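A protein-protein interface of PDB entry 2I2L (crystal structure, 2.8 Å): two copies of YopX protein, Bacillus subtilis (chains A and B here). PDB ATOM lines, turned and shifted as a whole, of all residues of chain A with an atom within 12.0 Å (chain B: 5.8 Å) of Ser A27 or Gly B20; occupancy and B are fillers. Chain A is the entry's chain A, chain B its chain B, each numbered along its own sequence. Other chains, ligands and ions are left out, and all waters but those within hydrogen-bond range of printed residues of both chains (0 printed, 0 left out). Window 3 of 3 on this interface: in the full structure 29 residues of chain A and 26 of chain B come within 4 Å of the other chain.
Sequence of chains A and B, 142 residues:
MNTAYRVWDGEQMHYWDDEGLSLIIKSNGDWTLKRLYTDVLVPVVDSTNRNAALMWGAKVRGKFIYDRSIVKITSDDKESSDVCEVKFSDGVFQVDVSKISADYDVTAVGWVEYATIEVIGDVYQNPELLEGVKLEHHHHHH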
ATOM      1  N   LEU A  23     -11.079  22.753 -34.638  1.00  0.00           N
ATOM      2  CA  LEU A  23     -11.011  23.955 -33.832  1.00  0.00           C
ATOM      3  C   LEU A  23     -11.955  23.810 -32.642  1.00  0.00           C
ATOM      4  O   LEU A  23     -13.062  23.268 -32.765  1.00  0.00           O
ATOM      5  CB  LEU A  23     -11.411  25.155 -34.678  1.00  0.00           C
ATOM      6  CG  LEU A  23     -11.353  26.509 -33.989  1.00  0.00           C
ATOM      7  CD1 LEU A  23      -9.963  26.721 -33.360  1.00  0.00           C
ATOM      8  CD2 LEU A  23     -11.693  27.583 -35.023  1.00  0.00           C
ATOM      9  N   ILE A  24     -11.517  24.282 -31.484  1.00  0.00           N
ATOM     10  CA  ILE A  24     -12.350  24.190 -30.294  1.00  0.00           C
ATOM     11  C   ILE A  24     -12.430  25.529 -29.573  1.00  0.00           C
ATOM     12  O   ILE A  24     -11.434  26.009 -29.013  1.00  0.00           O
ATOM     13  CB  ILE A  24     -11.822  23.127 -29.306  1.00  0.00           C
ATOM     14  CG1 ILE A  24     -11.905  21.739 -29.938  1.00  0.00           C
ATOM     15  CG2 ILE A  24     -12.611  23.178 -28.016  1.00  0.00           C
ATOM     16  CD1 ILE A  24     -10.812  21.453 -30.967  1.00  0.00           C
ATOM     17  N   ILE A  25     -13.618  26.126 -29.607  1.00  0.00           N
ATOM     18  CA  ILE A  25     -13.855  27.398 -28.949  1.00  0.00           C
ATOM     19  C   ILE A  25     -14.415  27.104 -27.562  1.00  0.00           C
ATOM     20  O   ILE A  25     -15.357  26.319 -27.433  1.00  0.00           O
ATOM     21  CB  ILE A  25     -14.853  28.247 -29.742  1.00  0.00           C
ATOM     22  CG1 ILE A  25     -14.235  28.641 -31.085  1.00  0.00           C
ATOM     23  CG2 ILE A  25     -15.232  29.486 -28.937  1.00  0.00           C
ATOM     24  CD1 ILE A  25     -15.101  29.573 -31.907  1.00  0.00           C
ATOM     25  N   LYS A  26     -13.842  27.714 -26.523  1.00  0.00           N
ATOM     26  CA  LYS A  26     -14.320  27.463 -25.161  1.00  0.00           C
ATOM     27  C   LYS A  26     -15.238  28.539 -24.573  1.00  0.00           C
ATOM     28  O   LYS A  26     -15.247  29.693 -25.011  1.00  0.00           O
ATOM     29  CB  LYS A  26     -13.138  27.221 -24.208  1.00  0.00           C
ATOM     30  CG  LYS A  26     -12.450  25.857 -24.352  1.00  0.00           C
ATOM     31  CD  LYS A  26     -13.384  24.706 -23.966  1.00  0.00           C
ATOM     32  CE  LYS A  26     -12.678  23.335 -24.012  1.00  0.00           C
ATOM     33  NZ  LYS A  26     -13.581  22.202 -23.573  1.00  0.00           N
ATOM     34  N   SER A  27     -15.998  28.125 -23.564  1.00  0.00           N
ATOM     35  CA  SER A  27     -16.963  28.973 -22.862  1.00  0.00           C
ATOM     36  C   SER A  27     -16.413  30.327 -22.435  1.00  0.00           C
ATOM     37  O   SER A  27     -17.163  31.289 -22.284  1.00  0.00           O
ATOM     38  CB  SER A  27     -17.494  28.244 -21.620  1.00  0.00           C
ATOM     39  OG  SER A  27     -18.054  26.975 -21.944  1.00  0.00           O
ATOM     40  N   ASN A  28     -15.104  30.399 -22.238  1.00  0.00           N
ATOM     41  CA  ASN A  28     -14.478  31.640 -21.809  1.00  0.00           C
ATOM     42  C   ASN A  28     -13.932  32.424 -23.003  1.00  0.00           C
ATOM     43  O   ASN A  28     -13.102  33.330 -22.837  1.00  0.00           O
ATOM     44  CB  ASN A  28     -13.336  31.328 -20.848  1.00  0.00           C
ATOM     45  CG  ASN A  28     -12.067  30.949 -21.572  1.00  0.00           C
ATOM     46  OD1 ASN A  28     -12.081  30.107 -22.473  1.00  0.00           O
ATOM     47  ND2 ASN A  28     -10.958  31.577 -21.189  1.00  0.00           N
ATOM     48  N   GLY A  29     -14.378  32.061 -24.202  1.00  0.00           N
ATOM     49  CA  GLY A  29     -13.923  32.759 -25.390  1.00  0.00           C
ATOM     50  C   GLY A  29     -12.599  32.283 -25.953  1.00  0.00           C
ATOM     51  O   GLY A  29     -12.253  32.622 -27.081  1.00  0.00           O
ATOM     52  N   ASP A  30     -11.843  31.514 -25.179  1.00  0.00           N
ATOM     53  CA  ASP A  30     -10.562  31.001 -25.661  1.00  0.00           C
ATOM     54  C   ASP A  30     -10.790  30.029 -26.811  1.00  0.00           C
ATOM     55  O   ASP A  30     -11.876  29.453 -26.946  1.00  0.00           O
ATOM     56  CB  ASP A  30      -9.833  30.252 -24.542  1.00  0.00           C
ATOM     57  CG  ASP A  30      -9.143  31.183 -23.555  1.00  0.00           C
ATOM     58  OD1 ASP A  30      -9.654  32.299 -23.306  1.00  0.00           O
ATOM     59  OD2 ASP A  30      -8.088  30.783 -23.014  1.00  0.00           O
ATOM     60  N   TRP A  31      -9.773  29.866 -27.652  1.00  0.00           N
ATOM     61  CA  TRP A  31      -9.854  28.914 -28.748  1.00  0.00           C
ATOM     62  C   TRP A  31      -8.606  28.045 -28.708  1.00  0.00           C
ATOM     63  O   TRP A  31      -7.628  28.385 -28.041  1.00  0.00           O
ATOM     64  CB  TRP A  31     -10.002  29.614 -30.105  1.00  0.00           C
ATOM     65  CG  TRP A  31      -8.879  30.508 -30.521  1.00  0.00           C
ATOM     66  CD1 TRP A  31      -8.866  31.870 -30.497  1.00  0.00           C
ATOM     67  CD2 TRP A  31      -7.622  30.104 -31.076  1.00  0.00           C
ATOM     68  NE1 TRP A  31      -7.679  32.341 -31.002  1.00  0.00           N
ATOM     69  CE2 TRP A  31      -6.898  31.280 -31.364  1.00  0.00           C
ATOM     70  CE3 TRP A  31      -7.039  28.862 -31.357  1.00  0.00           C
ATOM     71  CZ2 TRP A  31      -5.622  31.256 -31.922  1.00  0.00           C
ATOM     72  CZ3 TRP A  31      -5.769  28.836 -31.914  1.00  0.00           C
ATOM     73  CH2 TRP A  31      -5.071  30.030 -32.191  1.00  0.00           C
ATOM     74  N   THR A  32      -8.644  26.915 -29.403  1.00  0.00           N
ATOM     75  CA  THR A  32      -7.513  25.994 -29.417  1.00  0.00           C
ATOM     76  C   THR A  32      -7.547  25.125 -30.660  1.00  0.00           C
ATOM     77  O   THR A  32      -8.522  24.424 -30.900  1.00  0.00           O
ATOM     78  CB  THR A  32      -7.559  25.059 -28.197  1.00  0.00           C
ATOM     79  OG1 THR A  32      -7.484  25.828 -26.985  1.00  0.00           O
ATOM     80  CG2 THR A  32      -6.415  24.053 -28.270  1.00  0.00           C
ATOM     81  N   ASP A  46      -2.578  27.663 -29.552  1.00  0.00           N
ATOM     82  CA  ASP A  46      -3.668  28.050 -28.673  1.00  0.00           C
ATOM     83  C   ASP A  46      -3.769  29.553 -28.443  1.00  0.00           C
ATOM     84  O   ASP A  46      -2.764  30.234 -28.339  1.00  0.00           O
ATOM     85  CB  ASP A  46      -3.470  27.322 -27.350  1.00  0.00           C
ATOM     86  CG  ASP A  46      -4.192  27.977 -26.218  1.00  0.00           C
ATOM     87  OD1 ASP A  46      -5.448  28.023 -26.257  1.00  0.00           O
ATOM     88  OD2 ASP A  46      -3.494  28.450 -25.292  1.00  0.00           O
ATOM     89  N   SER A  47      -4.990  30.059 -28.330  1.00  0.00           N
ATOM     90  CA  SER A  47      -5.231  31.488 -28.134  1.00  0.00           C
ATOM     91  C   SER A  47      -4.425  32.212 -27.039  1.00  0.00           C
ATOM     92  O   SER A  47      -4.221  33.423 -27.130  1.00  0.00           O
ATOM     93  CB  SER A  47      -6.720  31.738 -27.879  1.00  0.00           C
ATOM     94  OG  SER A  47      -7.041  31.534 -26.513  1.00  0.00           O
ATOM     95  N   THR A  48      -3.979  31.514 -25.999  1.00  0.00           N
ATOM     96  CA  THR A  48      -3.220  32.211 -24.966  1.00  0.00           C
ATOM     97  C   THR A  48      -1.861  32.602 -25.530  1.00  0.00           C
ATOM     98  O   THR A  48      -1.143  33.389 -24.923  1.00  0.00           O
ATOM     99  CB  THR A  48      -3.012  31.365 -23.673  1.00  0.00           C
ATOM    100  OG1 THR A  48      -2.010  30.366 -23.893  1.00  0.00           O
ATOM    101  CG2 THR A  48      -4.325  30.702 -23.249  1.00  0.00           C
ATOM    102  N   TRP B  16     -22.399  30.982 -26.351  1.00  0.00           N
ATOM    103  CA  TRP B  16     -21.003  30.615 -26.103  1.00  0.00           C
ATOM    104  C   TRP B  16     -20.523  30.793 -24.665  1.00  0.00           C
ATOM    105  O   TRP B  16     -19.738  29.987 -24.157  1.00  0.00           O
ATOM    106  CB  TRP B  16     -20.085  31.410 -27.036  1.00  0.00           C
ATOM    107  CG  TRP B  16     -20.140  32.883 -26.794  1.00  0.00           C
ATOM    108  CD1 TRP B  16     -21.044  33.767 -27.306  1.00  0.00           C
ATOM    109  CD2 TRP B  16     -19.303  33.633 -25.907  1.00  0.00           C
ATOM    110  NE1 TRP B  16     -20.824  35.020 -26.789  1.00  0.00           N
ATOM    111  CE2 TRP B  16     -19.759  34.967 -25.923  1.00  0.00           C
ATOM    112  CE3 TRP B  16     -18.209  33.305 -25.090  1.00  0.00           C
ATOM    113  CZ2 TRP B  16     -19.161  35.982 -25.155  1.00  0.00           C
ATOM    114  CZ3 TRP B  16     -17.612  34.316 -24.322  1.00  0.00           C
ATOM    115  CH2 TRP B  16     -18.093  35.635 -24.363  1.00  0.00           C
ATOM    116  N   ASP B  17     -20.995  31.845 -24.010  1.00  0.00           N
ATOM    117  CA  ASP B  17     -20.587  32.108 -22.643  1.00  0.00           C
ATOM    118  C   ASP B  17     -21.226  31.200 -21.578  1.00  0.00           C
ATOM    119  O   ASP B  17     -20.729  31.146 -20.453  1.00  0.00           O
ATOM    120  CB  ASP B  17     -20.827  33.583 -22.325  1.00  0.00           C
ATOM    121  CG  ASP B  17     -22.186  34.048 -22.766  1.00  0.00           C
ATOM    122  OD1 ASP B  17     -23.169  33.828 -22.025  1.00  0.00           O
ATOM    123  OD2 ASP B  17     -22.276  34.621 -23.869  1.00  0.00           O
ATOM    124  N   ASP B  18     -22.300  30.482 -21.918  1.00  0.00           N
ATOM    125  CA  ASP B  18     -22.944  29.576 -20.956  1.00  0.00           C
ATOM    126  C   ASP B  18     -21.915  28.600 -20.361  1.00  0.00           C
ATOM    127  O   ASP B  18     -21.106  28.018 -21.090  1.00  0.00           O
ATOM    128  CB  ASP B  18     -24.043  28.724 -21.613  1.00  0.00           C
ATOM    129  CG  ASP B  18     -25.123  29.545 -22.298  1.00  0.00           C
ATOM    130  OD1 ASP B  18     -25.586  30.556 -21.724  1.00  0.00           O
ATOM    131  OD2 ASP B  18     -25.525  29.154 -23.414  1.00  0.00           O
ATOM    132  N   GLU B  19     -21.968  28.385 -19.049  1.00  0.00           N
ATOM    133  CA  GLU B  19     -21.026  27.483 -18.392  1.00  0.00           C
ATOM    134  C   GLU B  19     -20.828  26.121 -19.076  1.00  0.00           C
ATOM    135  O   GLU B  19     -21.794  25.417 -19.389  1.00  0.00           O
ATOM    136  CB  GLU B  19     -21.440  27.269 -16.931  1.00  0.00           C
ATOM    137  N   GLY B  20     -19.561  25.773 -19.306  1.00  0.00           N
ATOM    138  CA  GLY B  20     -19.206  24.489 -19.895  1.00  0.00           C
ATOM    139  C   GLY B  20     -19.444  24.181 -21.366  1.00  0.00           C
ATOM    140  O   GLY B  20     -19.142  23.067 -21.800  1.00  0.00           O
ATOM    141  N   LEU B  21     -19.972  25.123 -22.143  1.00  0.00           N
ATOM    142  CA  LEU B  21     -20.208  24.850 -23.552  1.00  0.00           C
ATOM    143  C   LEU B  21     -18.969  25.030 -24.393  1.00  0.00           C
ATOM    144  O   LEU B  21     -18.299  26.060 -24.313  1.00  0.00           O
ATOM    145  CB  LEU B  21     -21.294  25.758 -24.116  1.00  0.00           C
ATOM    146  CG  LEU B  21     -22.715  25.213 -24.116  1.00  0.00           C
ATOM    147  CD1 LEU B  21     -23.201  25.107 -22.672  1.00  0.00           C
ATOM    148  CD2 LEU B  21     -23.626  26.134 -24.943  1.00  0.00           C
ATOM    149  N   SER B  22     -18.664  24.034 -25.212  1.00  0.00           N
ATOM    150  CA  SER B  22     -17.518  24.142 -26.098  1.00  0.00           C
ATOM    151  C   SER B  22     -17.961  23.751 -27.501  1.00  0.00           C
ATOM    152  O   SER B  22     -18.495  22.668 -27.708  1.00  0.00           O
ATOM    153  CB  SER B  22     -16.379  23.230 -25.641  1.00  0.00           C
ATOM    154  OG  SER B  22     -16.601  21.889 -26.041  1.00  0.00           O
ATOM    155  N   LYS B  34     -20.546  20.796 -27.522  1.00  0.00           N
ATOM    156  CA  LYS B  34     -20.275  19.915 -26.391  1.00  0.00           C
ATOM    157  C   LYS B  34     -20.535  20.698 -25.104  1.00  0.00           C
ATOM    158  O   LYS B  34     -20.658  21.924 -25.131  1.00  0.00           O
ATOM    159  CB  LYS B  34     -18.818  19.437 -26.394  1.00  0.00           C
ATOM    160  CG  LYS B  34     -18.381  18.666 -27.634  1.00  0.00           C
ATOM    161  CD  LYS B  34     -19.209  17.409 -27.842  1.00  0.00           C
ATOM    162  CE  LYS B  34     -18.538  16.456 -28.826  1.00  0.00           C
ATOM    163  NZ  LYS B  34     -17.351  15.783 -28.228  1.00  0.00           N
ATOM    164  N   ARG B  35     -20.622  19.979 -23.986  1.00  0.00           N
ATOM    165  CA  ARG B  35     -20.847  20.578 -22.676  1.00  0.00           C
ATOM    166  C   ARG B  35     -20.173  19.709 -21.616  1.00  0.00           C
ATOM    167  O   ARG B  35     -20.403  18.502 -21.541  1.00  0.00           O
ATOM    168  CB  ARG B  35     -22.345  20.684 -22.388  1.00  0.00           C
ATOM    169  CG  ARG B  35     -22.668  21.007 -20.934  1.00  0.00           C
ATOM    170  CD  ARG B  35     -24.145  20.751 -20.597  1.00  0.00           C
ATOM    171  NE  ARG B  35     -25.040  21.799 -21.085  1.00  0.00           N
ATOM    172  CZ  ARG B  35     -25.048  23.054 -20.632  1.00  0.00           C
ATOM    173  NH1 ARG B  35     -24.207  23.431 -19.673  1.00  0.00           N
ATOM    174  NH2 ARG B  35     -25.896  23.941 -21.144  1.00  0.00           N
ATOM    175  N   LEU B  36     -19.330  20.333 -20.802  1.00  0.00           N
ATOM    176  CA  LEU B  36     -18.611  19.632 -19.748  1.00  0.00           C
ATOM    177  C   LEU B  36     -19.454  19.587 -18.472  1.00  0.00           C
ATOM    178  O   LEU B  36     -19.786  20.626 -17.892  1.00  0.00           O
ATOM    179  CB  LEU B  36     -17.273  20.333 -19.493  1.00  0.00           C
ATOM    180  CG  LEU B  36     -16.211  19.551 -18.726  1.00  0.00           C
ATOM    181  CD1 LEU B  36     -16.688  19.333 -17.315  1.00  0.00           C
ATOM    182  CD2 LEU B  36     -15.934  18.224 -19.411  1.00  0.00           C
ATOM    183  N   LEU B  41     -16.917  15.417 -21.141  1.00  0.00           N
ATOM    184  CA  LEU B  41     -17.445  16.155 -22.282  1.00  0.00           C
ATOM    185  C   LEU B  41     -18.694  15.463 -22.815  1.00  0.00           C
ATOM    186  O   LEU B  41     -18.619  14.338 -23.314  1.00  0.00           O
ATOM    187  CB  LEU B  41     -16.374  16.243 -23.377  1.00  0.00           C
ATOM    188  CG  LEU B  41     -15.954  17.657 -23.800  1.00  0.00           C
ATOM    189  CD1 LEU B  41     -15.798  18.543 -22.575  1.00  0.00           C
ATOM    190  CD2 LEU B  41     -14.651  17.590 -24.585  1.00  0.00           C
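The backbone carbonyl oxygen (O) of Ser A27 lies close to the backbone carbonyl oxygen (O) of Trp B16 (3.4 Å).
N of Gly B20 lies close to OG of Ser A27 (3.3 Å).
The side-chain hydroxyl (OG) of Ser A27 is in hydrogen-bond range of the backbone carbonyl oxygen (O) of Leu B21 (2.6 Å).
OG of Ser A27 is in hydrogen-bond range of O of Asp B18.
N of Lys B34 lies within hydrogen-bond range of O of Ser B22 (2.8 Å).
The backbone carbonyl oxygen of Gly B20 lies within hydrogen-bond range of the backbone NH of Leu B36 (2.9 Å).
OD2 of Asp B17 lies close to NE1 of Trp B16 (3.3 Å).
Among the printed residues, merely in contact across the chains: Ile A25 with Ser B22, Lys A26 with Leu B21, Lys A26 with Ser B22, Ser A27 with Asp B17 and Gly A29 with Trp B16.
Ser A27 touches five residues of chain B.
Gly B20 touches just one residue of chain A: Ser A27 (3.2 Å).
Trp B16 touches just these residues of chain A: Ser A27 (3.2 Å) and Gly A29 (3.9 Å).
Asp B17 touches just one residue of chain A: Ser A27 (3.5 Å).
Glu B19 touches none of the printed residues of chain A.
Of chain A, only Lys A26 and Ser A27 come within 4 Å of Leu B21.
Of chain A, only Ile A25 (3.3 Å) and Lys A26 (3.6 Å) come within 4 Å of Ser B22.
Arg B35 touches none of the printed residues of chain A.
Printed residues of chain B within 4 Å of Lys A26: Leu B21 (3.9 Å) and Ser B22 (3.6 Å).
Of the printed residues of chain B, Ile A25 touches Ser B22 (3.3 Å).
Printed residues of chain A within 4 Å of Asp B18: Ser A27.
The nearest residue of chain B that does not touch Ser A27 is Glu B19 (4.1 Å).
The nearest printed residue of chain B that does not touch Gly A29 is Asp B17 (6.4 Å).
Of the 13 printed residues of chain A, 4 touch a printed residue of chain B.
Hydrophobic or aromatic side chains of chain B within 4 Å of the printed part of chain A: Trp B16.
Among the printed residues, 9 pairs touch across the chains.
No position is printed for both chains.
Of the 9 pairs that touch across the chains among the printed residues, none has its exchanged pair printed and touching as well.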
